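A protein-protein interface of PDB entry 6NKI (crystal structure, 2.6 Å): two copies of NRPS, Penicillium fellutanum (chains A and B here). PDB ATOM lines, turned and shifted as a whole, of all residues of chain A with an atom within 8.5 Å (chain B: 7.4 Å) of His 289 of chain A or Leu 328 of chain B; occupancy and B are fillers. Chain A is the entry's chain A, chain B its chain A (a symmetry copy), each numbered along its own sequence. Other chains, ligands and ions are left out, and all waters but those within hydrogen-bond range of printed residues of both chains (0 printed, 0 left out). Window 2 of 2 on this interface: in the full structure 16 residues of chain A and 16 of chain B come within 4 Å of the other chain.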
ATOM      1  N   LYS A  22       3.883   4.771 -21.944  1.00  0.00           N
ATOM      2  CA  LYS A  22       2.608   5.389 -22.301  1.00  0.00           C
ATOM      3  C   LYS A  22       2.354   6.627 -21.452  1.00  0.00           C
ATOM      4  O   LYS A  22       2.456   6.578 -20.225  1.00  0.00           O
ATOM      5  CB  LYS A  22       1.452   4.409 -22.122  1.00  0.00           C
ATOM      6  CG  LYS A  22       1.413   3.249 -23.091  1.00  0.00           C
ATOM      7  CD  LYS A  22       0.900   3.692 -24.450  1.00  0.00           C
ATOM      8  CE  LYS A  22       0.586   2.499 -25.334  1.00  0.00           C
ATOM      9  NZ  LYS A  22      -0.008   2.936 -26.620  1.00  0.00           N
ATOM     10  N   LEU A  41      -4.914   3.110 -14.129  1.00  0.00           N
ATOM     11  CA  LEU A  41      -3.819   3.496 -15.028  1.00  0.00           C
ATOM     12  C   LEU A  41      -2.473   3.364 -14.329  1.00  0.00           C
ATOM     13  O   LEU A  41      -1.596   2.632 -14.786  1.00  0.00           O
ATOM     14  CB  LEU A  41      -4.012   4.924 -15.539  1.00  0.00           C
ATOM     15  CG  LEU A  41      -5.189   5.077 -16.483  1.00  0.00           C
ATOM     16  CD1 LEU A  41      -5.455   6.538 -16.717  1.00  0.00           C
ATOM     17  CD2 LEU A  41      -4.918   4.350 -17.786  1.00  0.00           C
ATOM     18  N   ASP A  44      -1.135  -0.187 -14.251  1.00  0.00           N
ATOM     19  CA  ASP A  44      -0.669  -0.753 -15.511  1.00  0.00           C
ATOM     20  C   ASP A  44       0.790  -0.375 -15.747  1.00  0.00           C
ATOM     21  O   ASP A  44       1.239   0.715 -15.383  1.00  0.00           O
ATOM     22  CB  ASP A  44      -1.522  -0.269 -16.689  1.00  0.00           C
ATOM     23  CG  ASP A  44      -1.110  -0.919 -18.020  1.00  0.00           C
ATOM     24  OD1 ASP A  44      -1.539  -2.061 -18.288  1.00  0.00           O
ATOM     25  OD2 ASP A  44      -0.323  -0.314 -18.783  1.00  0.00           O
ATOM     26  N   ASN A  45       1.536  -1.289 -16.375  1.00  0.00           N
ATOM     27  CA  ASN A  45       2.967  -1.074 -16.561  1.00  0.00           C
ATOM     28  C   ASN A  45       3.292  -0.198 -17.764  1.00  0.00           C
ATOM     29  O   ASN A  45       4.330   0.474 -17.761  1.00  0.00           O
ATOM     30  CB  ASN A  45       3.697  -2.415 -16.690  1.00  0.00           C
ATOM     31  CG  ASN A  45       3.958  -3.078 -15.347  1.00  0.00           C
ATOM     32  OD1 ASN A  45       4.403  -2.427 -14.400  1.00  0.00           O
ATOM     33  ND2 ASN A  45       3.686  -4.380 -15.262  1.00  0.00           N
ATOM     34  N   ASP A  46       2.448  -0.190 -18.803  1.00  0.00           N
ATOM     35  CA  ASP A  46       2.790   0.585 -19.995  1.00  0.00           C
ATOM     36  C   ASP A  46       2.737   2.086 -19.743  1.00  0.00           C
ATOM     37  O   ASP A  46       3.534   2.834 -20.320  1.00  0.00           O
ATOM     38  CB  ASP A  46       1.879   0.232 -21.173  1.00  0.00           C
ATOM     39  CG  ASP A  46       2.267  -1.065 -21.847  1.00  0.00           C
ATOM     40  OD1 ASP A  46       3.456  -1.450 -21.763  1.00  0.00           O
ATOM     41  OD2 ASP A  46       1.392  -1.683 -22.487  1.00  0.00           O
ATOM     42  N   VAL A  47       1.818   2.544 -18.892  1.00  0.00           N
ATOM     43  CA  VAL A  47       1.625   3.975 -18.708  1.00  0.00           C
ATOM     44  C   VAL A  47       2.816   4.568 -17.960  1.00  0.00           C
ATOM     45  O   VAL A  47       3.226   4.073 -16.902  1.00  0.00           O
ATOM     46  CB  VAL A  47       0.286   4.245 -18.006  1.00  0.00           C
ATOM     47  CG1 VAL A  47       0.251   3.570 -16.695  1.00  0.00           C
ATOM     48  CG2 VAL A  47       0.086   5.734 -17.814  1.00  0.00           C
ATOM     49  N   ALA A 162      -5.261   8.087 -28.774  1.00  0.00           N
ATOM     50  CA  ALA A 162      -6.527   7.417 -28.487  1.00  0.00           C
ATOM     51  C   ALA A 162      -7.433   8.294 -27.618  1.00  0.00           C
ATOM     52  O   ALA A 162      -6.999   8.852 -26.602  1.00  0.00           O
ATOM     53  CB  ALA A 162      -6.276   6.072 -27.804  1.00  0.00           C
ATOM     54  N   SER A 225      -7.932   5.891 -32.834  1.00  0.00           N
ATOM     55  CA  SER A 225      -8.802   4.898 -32.214  1.00  0.00           C
ATOM     56  C   SER A 225      -9.646   5.617 -31.170  1.00  0.00           C
ATOM     57  O   SER A 225      -9.119   6.132 -30.177  1.00  0.00           O
ATOM     58  CB  SER A 225      -7.990   3.771 -31.584  1.00  0.00           C
ATOM     59  OG  SER A 225      -7.369   4.199 -30.384  1.00  0.00           O
ATOM     60  N   SER A 281     -12.038  -0.636 -15.439  1.00  0.00           N
ATOM     61  CA  SER A 281     -11.236  -1.630 -16.148  1.00  0.00           C
ATOM     62  C   SER A 281     -11.609  -1.666 -17.622  1.00  0.00           C
ATOM     63  O   SER A 281     -10.741  -1.716 -18.508  1.00  0.00           O
ATOM     64  CB  SER A 281     -11.429  -3.026 -15.514  1.00  0.00           C
ATOM     65  OG  SER A 281     -10.659  -4.066 -16.148  1.00  0.00           O
ATOM     66  N   LEU A 282     -12.914  -1.636 -17.903  1.00  0.00           N
ATOM     67  CA  LEU A 282     -13.376  -1.682 -19.282  1.00  0.00           C
ATOM     68  C   LEU A 282     -13.021  -0.415 -20.059  1.00  0.00           C
ATOM     69  O   LEU A 282     -12.972  -0.464 -21.281  1.00  0.00           O
ATOM     70  CB  LEU A 282     -14.889  -1.932 -19.322  1.00  0.00           C
ATOM     71  CG  LEU A 282     -15.558  -1.970 -20.704  1.00  0.00           C
ATOM     72  CD1 LEU A 282     -14.845  -2.996 -21.574  1.00  0.00           C
ATOM     73  CD2 LEU A 282     -17.028  -2.310 -20.636  1.00  0.00           C
ATOM     74  N   ILE A 283     -12.792   0.714 -19.386  1.00  0.00           N
ATOM     75  CA  ILE A 283     -12.429   1.927 -20.107  1.00  0.00           C
ATOM     76  C   ILE A 283     -10.966   1.881 -20.507  1.00  0.00           C
ATOM     77  O   ILE A 283     -10.611   2.237 -21.637  1.00  0.00           O
ATOM     78  CB  ILE A 283     -12.759   3.187 -19.275  1.00  0.00           C
ATOM     79  CG1 ILE A 283     -14.282   3.440 -19.229  1.00  0.00           C
ATOM     80  CG2 ILE A 283     -12.036   4.389 -19.842  1.00  0.00           C
ATOM     81  CD1 ILE A 283     -14.747   4.284 -18.059  1.00  0.00           C
ATOM     82  N   ILE A 284     -10.124   1.476 -19.563  1.00  0.00           N
ATOM     83  CA  ILE A 284      -8.660   1.401 -19.803  1.00  0.00           C
ATOM     84  C   ILE A 284      -8.368   0.383 -20.901  1.00  0.00           C
ATOM     85  O   ILE A 284      -7.588   0.696 -21.778  1.00  0.00           O
ATOM     86  CB  ILE A 284      -7.937   1.056 -18.499  1.00  0.00           C
ATOM     87  CG1 ILE A 284      -8.097   2.181 -17.479  1.00  0.00           C
ATOM     88  CG2 ILE A 284      -6.482   0.736 -18.770  1.00  0.00           C
ATOM     89  CD1 ILE A 284      -7.340   1.953 -16.203  1.00  0.00           C
ATOM     90  N   HIS A 285      -9.012  -0.774 -20.891  1.00  0.00           N
ATOM     91  CA  HIS A 285      -8.703  -1.753 -21.962  1.00  0.00           C
ATOM     92  C   HIS A 285      -9.093  -1.173 -23.318  1.00  0.00           C
ATOM     93  O   HIS A 285      -8.322  -1.320 -24.264  1.00  0.00           O
ATOM     94  CB  HIS A 285      -9.431  -3.074 -21.721  1.00  0.00           C
ATOM     95  CG  HIS A 285      -9.440  -3.965 -22.913  1.00  0.00           C
ATOM     96  ND1 HIS A 285      -8.429  -4.858 -23.166  1.00  0.00           N
ATOM     97  CD2 HIS A 285     -10.325  -4.101 -23.918  1.00  0.00           C
ATOM     98  CE1 HIS A 285      -8.696  -5.513 -24.270  1.00  0.00           C
ATOM     99  NE2 HIS A 285      -9.847  -5.064 -24.754  1.00  0.00           N
ATOM    100  N   GLU A 286     -10.251  -0.527 -23.388  1.00  0.00           N
ATOM    101  CA  GLU A 286     -10.743   0.045 -24.663  1.00  0.00           C
ATOM    102  C   GLU A 286      -9.787   1.130 -25.160  1.00  0.00           C
ATOM    103  O   GLU A 286      -9.563   1.196 -26.367  1.00  0.00           O
ATOM    104  CB  GLU A 286     -12.157   0.588 -24.489  1.00  0.00           C
ATOM    105  CG  GLU A 286     -13.206  -0.489 -24.624  1.00  0.00           C
ATOM    106  CD  GLU A 286     -12.903  -1.462 -25.744  1.00  0.00           C
ATOM    107  OE1 GLU A 286     -12.181  -1.072 -26.661  1.00  0.00           O
ATOM    108  OE2 GLU A 286     -13.384  -2.606 -25.688  1.00  0.00           O
ATOM    109  N   THR A 287      -9.243   1.952 -24.267  1.00  0.00           N
ATOM    110  CA  THR A 287      -8.338   3.023 -24.744  1.00  0.00           C
ATOM    111  C   THR A 287      -6.881   2.556 -24.789  1.00  0.00           C
ATOM    112  O   THR A 287      -6.055   3.349 -25.230  1.00  0.00           O
ATOM    113  CB  THR A 287      -8.464   4.295 -23.900  1.00  0.00           C
ATOM    114  OG1 THR A 287      -7.728   5.324 -24.549  1.00  0.00           O
ATOM    115  CG2 THR A 287      -8.001   4.118 -22.472  1.00  0.00           C
ATOM    116  N   LEU A 288      -6.555   1.344 -24.340  1.00  0.00           N
ATOM    117  CA  LEU A 288      -5.115   0.979 -24.368  1.00  0.00           C
ATOM    118  C   LEU A 288      -4.814  -0.326 -25.105  1.00  0.00           C
ATOM    119  O   LEU A 288      -3.714  -0.429 -25.637  1.00  0.00           O
ATOM    120  CB  LEU A 288      -4.591   0.867 -22.937  1.00  0.00           C
ATOM    121  CG  LEU A 288      -4.216   2.175 -22.259  1.00  0.00           C
ATOM    122  CD1 LEU A 288      -3.303   1.905 -21.078  1.00  0.00           C
ATOM    123  CD2 LEU A 288      -3.545   3.111 -23.239  1.00  0.00           C
ATOM    124  N   HIS A 289      -5.686  -1.327 -25.048  1.00  0.00           N
ATOM    125  CA  HIS A 289      -5.281  -2.618 -25.665  1.00  0.00           C
ATOM    126  C   HIS A 289      -6.328  -3.189 -26.619  1.00  0.00           C
ATOM    127  O   HIS A 289      -6.286  -4.394 -26.841  1.00  0.00           O
ATOM    128  CB  HIS A 289      -4.939  -3.634 -24.576  1.00  0.00           C
ATOM    129  CG  HIS A 289      -3.794  -3.245 -23.708  1.00  0.00           C
ATOM    130  ND1 HIS A 289      -3.967  -2.711 -22.459  1.00  0.00           N
ATOM    131  CD2 HIS A 289      -2.464  -3.322 -23.900  1.00  0.00           C
ATOM    132  CE1 HIS A 289      -2.795  -2.476 -21.914  1.00  0.00           C
ATOM    133  NE2 HIS A 289      -1.860  -2.842 -22.775  1.00  0.00           N
ATOM    134  N   ALA A 290      -7.253  -2.392 -27.136  1.00  0.00           N
ATOM    135  CA  ALA A 290      -8.234  -3.024 -28.043  1.00  0.00           C
ATOM    136  C   ALA A 290      -8.095  -2.438 -29.444  1.00  0.00           C
ATOM    137  O   ALA A 290      -8.236  -1.216 -29.592  1.00  0.00           O
ATOM    138  CB  ALA A 290      -9.624  -2.832 -27.511  1.00  0.00           C
ATOM    139  N   ARG A 291      -7.868  -3.301 -30.433  1.00  0.00           N
ATOM    140  CA  ARG A 291      -7.741  -2.844 -31.816  1.00  0.00           C
ATOM    141  C   ARG A 291      -6.621  -1.816 -31.975  1.00  0.00           C
ATOM    142  O   ARG A 291      -5.541  -1.966 -31.401  1.00  0.00           O
ATOM    143  CB  ARG A 291      -9.068  -2.265 -32.322  1.00  0.00           C
ATOM    144  CG  ARG A 291     -10.163  -3.298 -32.517  1.00  0.00           C
ATOM    145  CD  ARG A 291     -11.468  -2.650 -32.954  1.00  0.00           C
ATOM    146  NE  ARG A 291     -12.539  -3.632 -33.114  1.00  0.00           N
ATOM    147  CZ  ARG A 291     -13.806  -3.324 -33.375  1.00  0.00           C
ATOM    148  NH1 ARG A 291     -14.169  -2.055 -33.499  1.00  0.00           N
ATOM    149  NH2 ARG A 291     -14.712  -4.285 -33.502  1.00  0.00           N
ATOM    150  N   PHE B 322      -9.263 -15.228 -25.794  1.00  0.00           N
ATOM    151  CA  PHE B 322      -8.459 -15.832 -24.733  1.00  0.00           C
ATOM    152  C   PHE B 322      -6.962 -15.764 -25.060  1.00  0.00           C
ATOM    153  O   PHE B 322      -6.166 -15.215 -24.284  1.00  0.00           O
ATOM    154  CB  PHE B 322      -8.941 -17.280 -24.485  1.00  0.00           C
ATOM    155  CG  PHE B 322      -7.973 -18.124 -23.675  1.00  0.00           C
ATOM    156  CD1 PHE B 322      -7.819 -17.920 -22.313  1.00  0.00           C
ATOM    157  CD2 PHE B 322      -7.184 -19.098 -24.304  1.00  0.00           C
ATOM    158  CE1 PHE B 322      -6.912 -18.672 -21.576  1.00  0.00           C
ATOM    159  CE2 PHE B 322      -6.271 -19.837 -23.586  1.00  0.00           C
ATOM    160  CZ  PHE B 322      -6.147 -19.625 -22.199  1.00  0.00           C
ATOM    161  N   TRP B 323      -6.561 -16.276 -26.225  1.00  0.00           N
ATOM    162  CA  TRP B 323      -5.131 -16.318 -26.528  1.00  0.00           C
ATOM    163  C   TRP B 323      -4.513 -14.933 -26.708  1.00  0.00           C
ATOM    164  O   TRP B 323      -3.352 -14.736 -26.327  1.00  0.00           O
ATOM    165  CB  TRP B 323      -4.851 -17.149 -27.767  1.00  0.00           C
ATOM    166  CG  TRP B 323      -5.002 -18.609 -27.585  1.00  0.00           C
ATOM    167  CD1 TRP B 323      -5.973 -19.407 -28.109  1.00  0.00           C
ATOM    168  CD2 TRP B 323      -4.173 -19.452 -26.794  1.00  0.00           C
ATOM    169  NE1 TRP B 323      -5.774 -20.711 -27.725  1.00  0.00           N
ATOM    170  CE2 TRP B 323      -4.673 -20.761 -26.911  1.00  0.00           C
ATOM    171  CE3 TRP B 323      -3.042 -19.231 -26.007  1.00  0.00           C
ATOM    172  CZ2 TRP B 323      -4.074 -21.841 -26.287  1.00  0.00           C
ATOM    173  CZ3 TRP B 323      -2.456 -20.307 -25.378  1.00  0.00           C
ATOM    174  CH2 TRP B 323      -2.973 -21.588 -25.520  1.00  0.00           C
ATOM    175  N   LYS B 324      -5.242 -13.960 -27.275  1.00  0.00           N
ATOM    176  CA  LYS B 324      -4.599 -12.660 -27.386  1.00  0.00           C
ATOM    177  C   LYS B 324      -4.368 -12.054 -26.021  1.00  0.00           C
ATOM    178  O   LYS B 324      -3.501 -11.185 -25.884  1.00  0.00           O
ATOM    179  CB  LYS B 324      -5.363 -11.696 -28.306  1.00  0.00           C
ATOM    180  CG  LYS B 324      -6.790 -11.357 -27.979  1.00  0.00           C
ATOM    181  CD  LYS B 324      -7.290 -10.206 -28.890  1.00  0.00           C
ATOM    182  CE  LYS B 324      -7.537 -10.587 -30.367  1.00  0.00           C
ATOM    183  NZ  LYS B 324      -8.737 -11.445 -30.616  1.00  0.00           N
ATOM    184  N   ALA B 325      -5.086 -12.541 -25.001  1.00  0.00           N
ATOM    185  CA  ALA B 325      -4.880 -12.095 -23.633  1.00  0.00           C
ATOM    186  C   ALA B 325      -3.685 -12.792 -23.002  1.00  0.00           C
ATOM    187  O   ALA B 325      -2.891 -12.153 -22.303  1.00  0.00           O
ATOM    188  CB  ALA B 325      -6.152 -12.332 -22.824  1.00  0.00           C
ATOM    189  N   ILE B 326      -3.563 -14.108 -23.223  1.00  0.00           N
ATOM    190  CA  ILE B 326      -2.333 -14.833 -22.892  1.00  0.00           C
ATOM    191  C   ILE B 326      -1.113 -14.080 -23.430  1.00  0.00           C
ATOM    192  O   ILE B 326      -0.201 -13.699 -22.681  1.00  0.00           O
ATOM    193  CB  ILE B 326      -2.396 -16.275 -23.449  1.00  0.00           C
ATOM    194  CG1 ILE B 326      -3.492 -17.149 -22.767  1.00  0.00           C
ATOM    195  CG2 ILE B 326      -1.001 -16.916 -23.470  1.00  0.00           C
ATOM    196  CD1 ILE B 326      -3.265 -17.475 -21.252  1.00  0.00           C
ATOM    197  N   MET B 327      -1.092 -13.831 -24.740  1.00  0.00           N
ATOM    198  CA  MET B 327       0.094 -13.207 -25.325  1.00  0.00           C
ATOM    199  C   MET B 327       0.310 -11.798 -24.791  1.00  0.00           C
ATOM    200  O   MET B 327       1.459 -11.375 -24.613  1.00  0.00           O
ATOM    201  CB  MET B 327      -0.010 -13.177 -26.852  1.00  0.00           C
ATOM    202  CG  MET B 327       0.007 -14.541 -27.561  1.00  0.00           C
ATOM    203  SD  MET B 327      -0.137 -14.320 -29.335  1.00  0.00           S
ATOM    204  CE  MET B 327      -1.845 -13.854 -29.515  1.00  0.00           C
ATOM    205  N   LEU B 328      -0.774 -11.068 -24.518  1.00  0.00           N
ATOM    206  CA  LEU B 328      -0.649  -9.745 -23.920  1.00  0.00           C
ATOM    207  C   LEU B 328       0.022  -9.806 -22.552  1.00  0.00           C
ATOM    208  O   LEU B 328       0.830  -8.936 -22.209  1.00  0.00           O
ATOM    209  CB  LEU B 328      -2.026  -9.097 -23.810  1.00  0.00           C
ATOM    210  CG  LEU B 328      -2.116  -7.590 -23.527  1.00  0.00           C
ATOM    211  CD1 LEU B 328      -3.379  -7.053 -24.174  1.00  0.00           C
ATOM    212  CD2 LEU B 328      -2.087  -7.240 -22.031  1.00  0.00           C
ATOM    213  N   GLY B 329      -0.310 -10.829 -21.756  1.00  0.00           N
ATOM    214  CA  GLY B 329       0.299 -10.977 -20.445  1.00  0.00           C
ATOM    215  C   GLY B 329       1.691 -11.573 -20.508  1.00  0.00           C
ATOM    216  O   GLY B 329       2.594 -11.144 -19.778  1.00  0.00           O
ATOM    217  N   LEU B 330       1.891 -12.574 -21.375  1.00  0.00           N
ATOM    218  CA  LEU B 330       3.246 -13.079 -21.579  1.00  0.00           C
ATOM    219  C   LEU B 330       4.159 -11.999 -22.154  1.00  0.00           C
ATOM    220  O   LEU B 330       5.387 -12.066 -22.007  1.00  0.00           O
ATOM    221  CB  LEU B 330       3.235 -14.305 -22.501  1.00  0.00           C
ATOM    222  CG  LEU B 330       2.597 -15.648 -22.104  1.00  0.00           C
ATOM    223  CD1 LEU B 330       2.693 -16.646 -23.254  1.00  0.00           C
ATOM    224  CD2 LEU B 330       3.219 -16.223 -20.842  1.00  0.00           C
ATOM    225  N   GLY B 331       3.582 -10.994 -22.804  1.00  0.00           N
ATOM    226  CA  GLY B 331       4.393  -9.959 -23.400  1.00  0.00           C
ATOM    227  C   GLY B 331       5.159 -10.397 -24.621  1.00  0.00           C
ATOM    228  O   GLY B 331       6.200  -9.809 -24.935  1.00  0.00           O
ATOM    229  N   ARG B 332       4.671 -11.412 -25.325  1.00  0.00           N
ATOM    230  CA  ARG B 332       5.360 -11.933 -26.491  1.00  0.00           C
ATOM    231  C   ARG B 332       4.330 -12.636 -27.358  1.00  0.00           C
ATOM    232  O   ARG B 332       3.295 -13.093 -26.874  1.00  0.00           O
ATOM    233  CB  ARG B 332       6.486 -12.895 -26.093  1.00  0.00           C
ATOM    234  CG  ARG B 332       5.987 -14.251 -25.639  1.00  0.00           C
ATOM    235  CD  ARG B 332       7.104 -15.091 -25.052  1.00  0.00           C
ATOM    236  NE  ARG B 332       6.693 -16.482 -24.888  1.00  0.00           N
ATOM    237  CZ  ARG B 332       7.424 -17.409 -24.287  1.00  0.00           C
ATOM    238  NH1 ARG B 332       8.591 -17.086 -23.747  1.00  0.00           N
ATOM    239  NH2 ARG B 332       6.976 -18.648 -24.199  1.00  0.00           N
ATOM    240  N   ASP B 333       4.631 -12.734 -28.641  1.00  0.00           N
ATOM    241  CA  ASP B 333       3.705 -13.376 -29.559  1.00  0.00           C
ATOM    242  C   ASP B 333       4.010 -14.858 -29.708  1.00  0.00           C
ATOM    243  O   ASP B 333       5.158 -15.298 -29.589  1.00  0.00           O
ATOM    244  CB  ASP B 333       3.713 -12.678 -30.918  1.00  0.00           C
ATOM    245  CG  ASP B 333       3.066 -11.309 -30.854  1.00  0.00           C
ATOM    246  OD1 ASP B 333       2.202 -11.102 -29.958  1.00  0.00           O
ATOM    247  OD2 ASP B 333       3.409 -10.443 -31.695  1.00  0.00           O
ATOM    248  N   ARG B 396     -11.145 -11.445 -19.146  1.00  0.00           N
ATOM    249  CA  ARG B 396      -9.967 -11.120 -19.948  1.00  0.00           C
ATOM    250  C   ARG B 396      -8.815 -10.613 -19.102  1.00  0.00           C
ATOM    251  O   ARG B 396      -7.689 -11.086 -19.258  1.00  0.00           O
ATOM    252  CB  ARG B 396     -10.341 -10.134 -21.062  1.00  0.00           C
ATOM    253  CG  ARG B 396      -9.173  -9.390 -21.638  1.00  0.00           C
ATOM    254  CD  ARG B 396      -9.451  -8.619 -22.884  1.00  0.00           C
ATOM    255  NE  ARG B 396     -10.567  -7.685 -22.783  1.00  0.00           N
ATOM    256  CZ  ARG B 396     -11.690  -7.772 -23.506  1.00  0.00           C
ATOM    257  NH1 ARG B 396     -11.829  -8.673 -24.487  1.00  0.00           N
ATOM    258  NH2 ARG B 396     -12.680  -6.925 -23.256  1.00  0.00           N
ATOM    259  N   GLN B 397      -9.070  -9.708 -18.177  1.00  0.00           N
ATOM    260  CA  GLN B 397      -7.976  -9.269 -17.333  1.00  0.00           C
ATOM    261  C   GLN B 397      -7.552 -10.372 -16.375  1.00  0.00           C
ATOM    262  O   GLN B 397      -6.396 -10.417 -15.949  1.00  0.00           O
ATOM    263  CB  GLN B 397      -8.364  -7.998 -16.544  1.00  0.00           C
ATOM    264  CG  GLN B 397      -8.731  -6.843 -17.385  1.00  0.00           C
ATOM    265  CD  GLN B 397      -7.608  -6.403 -18.302  1.00  0.00           C
ATOM    266  OE1 GLN B 397      -7.702  -6.582 -19.512  1.00  0.00           O
ATOM    267  NE2 GLN B 397      -6.554  -5.802 -17.731  1.00  0.00           N
ATOM    268  N   VAL B 400      -5.140 -12.270 -18.475  1.00  0.00           N
ATOM    269  CA  VAL B 400      -3.950 -11.455 -18.685  1.00  0.00           C
ATOM    270  C   VAL B 400      -3.095 -11.444 -17.431  1.00  0.00           C
ATOM    271  O   VAL B 400      -1.870 -11.575 -17.493  1.00  0.00           O
ATOM    272  CB  VAL B 400      -4.308 -10.018 -19.128  1.00  0.00           C
ATOM    273  CG1 VAL B 400      -3.055  -9.122 -19.107  1.00  0.00           C
ATOM    274  CG2 VAL B 400      -4.876  -9.987 -20.541  1.00  0.00           C
ATOM    275  N   ARG B 401      -3.716 -11.263 -16.275  1.00  0.00           N
ATOM    276  CA  ARG B 401      -2.908 -11.156 -15.066  1.00  0.00           C
ATOM    277  C   ARG B 401      -2.267 -12.501 -14.720  1.00  0.00           C
ATOM    278  O   ARG B 401      -1.205 -12.543 -14.085  1.00  0.00           O
ATOM    279  CB  ARG B 401      -3.743 -10.653 -13.882  1.00  0.00           C
ATOM    280  CG  ARG B 401      -4.477  -9.329 -14.035  1.00  0.00           C
ATOM    281  CD  ARG B 401      -3.544  -8.167 -14.316  1.00  0.00           C
ATOM    282  NE  ARG B 401      -2.494  -8.010 -13.311  1.00  0.00           N
ATOM    283  CZ  ARG B 401      -2.642  -7.369 -12.155  1.00  0.00           C
ATOM    284  NH1 ARG B 401      -3.813  -6.828 -11.836  1.00  0.00           N
ATOM    285  NH2 ARG B 401      -1.617  -7.278 -11.317  1.00  0.00           N
ATOM    286  N   ALA B 403      -1.377 -14.979 -17.092  1.00  0.00           N
ATOM    287  CA  ALA B 403      -0.311 -15.211 -18.056  1.00  0.00           C
ATOM    288  C   ALA B 403       0.911 -14.341 -17.776  1.00  0.00           C
ATOM    289  O   ALA B 403       2.035 -14.725 -18.107  1.00  0.00           O
ATOM    290  CB  ALA B 403      -0.838 -14.961 -19.468  1.00  0.00           C
ATOM    291  N   GLU B 404       0.708 -13.155 -17.201  1.00  0.00           N
ATOM    292  CA  GLU B 404       1.818 -12.324 -16.741  1.00  0.00           C
ATOM    293  C   GLU B 404       2.487 -12.902 -15.495  1.00  0.00           C
ATOM    294  O   GLU B 404       3.662 -12.622 -15.239  1.00  0.00           O
ATOM    295  CB  GLU B 404       1.320 -10.904 -16.472  1.00  0.00           C
ATOM    296  CG  GLU B 404       2.384  -9.957 -15.917  1.00  0.00           C
ATOM    297  CD  GLU B 404       1.929  -8.504 -15.823  1.00  0.00           C
ATOM    298  OE1 GLU B 404       0.771  -8.202 -16.184  1.00  0.00           O
ATOM    299  OE2 GLU B 404       2.748  -7.660 -15.392  1.00  0.00           O
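Of the 18 printed residues of chain B, 4 touch a printed residue of chain A. Among the printed residues, 4 pairs touch across the chains. Among the printed residues, no Asp or Glu carboxylate lies within 4 Å of a Lys or Arg side-chain nitrogen of the other chain.
The side-chain carboxylate (OE2) of Glu 404 of chain B is in hydrogen-bond range of the side-chain amide nitrogen (ND2) of Asn 45 of chain A, 3.4 Å away. NE2 of His 285 of chain A sits close to NE of Arg 396 of chain B (3.4 Å).
No position is printed for both chains. Of the 4 pairs that touch across the chains among the printed residues, none has its exchanged pair printed and touching as well.
CG of Gln 397 of chain B touches OG of Ser 281 of chain A (3.6 Å). His 289 of chain A touches Leu 328 of chain B (CB to CD1, 3.8 Å).
Of the printed residues of chain B, Asn 45 of chain A touches Glu 404 (3.4 Å). Of the printed residues of chain B, Ser 281 of chain A touches Gln 397. Of the printed residues of chain B, His 285 of chain A touches Arg 396. His 289 of chain A touches one residue of chain B. Of the printed residues of chain A, Leu 328 of chain B touches His 289 (3.8 Å). Of the printed residues of chain A, Arg 396 of chain B touches His 285. Of the printed residues of chain A, Gln 397 of chain B touches Ser 281 (3.6 Å).
A ring nitrogen (NE2) of His 289 of chain A lies within hydrogen-bond range of the side-chain carboxylate (OD2) of Asp 46 of chain A (3.5 Å). The backbone carbonyl oxygen (O) of His 285 of chain A sits at hydrogen-bond distance from the backbone NH (N) of Ala 290 of chain A (3.2 Å).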
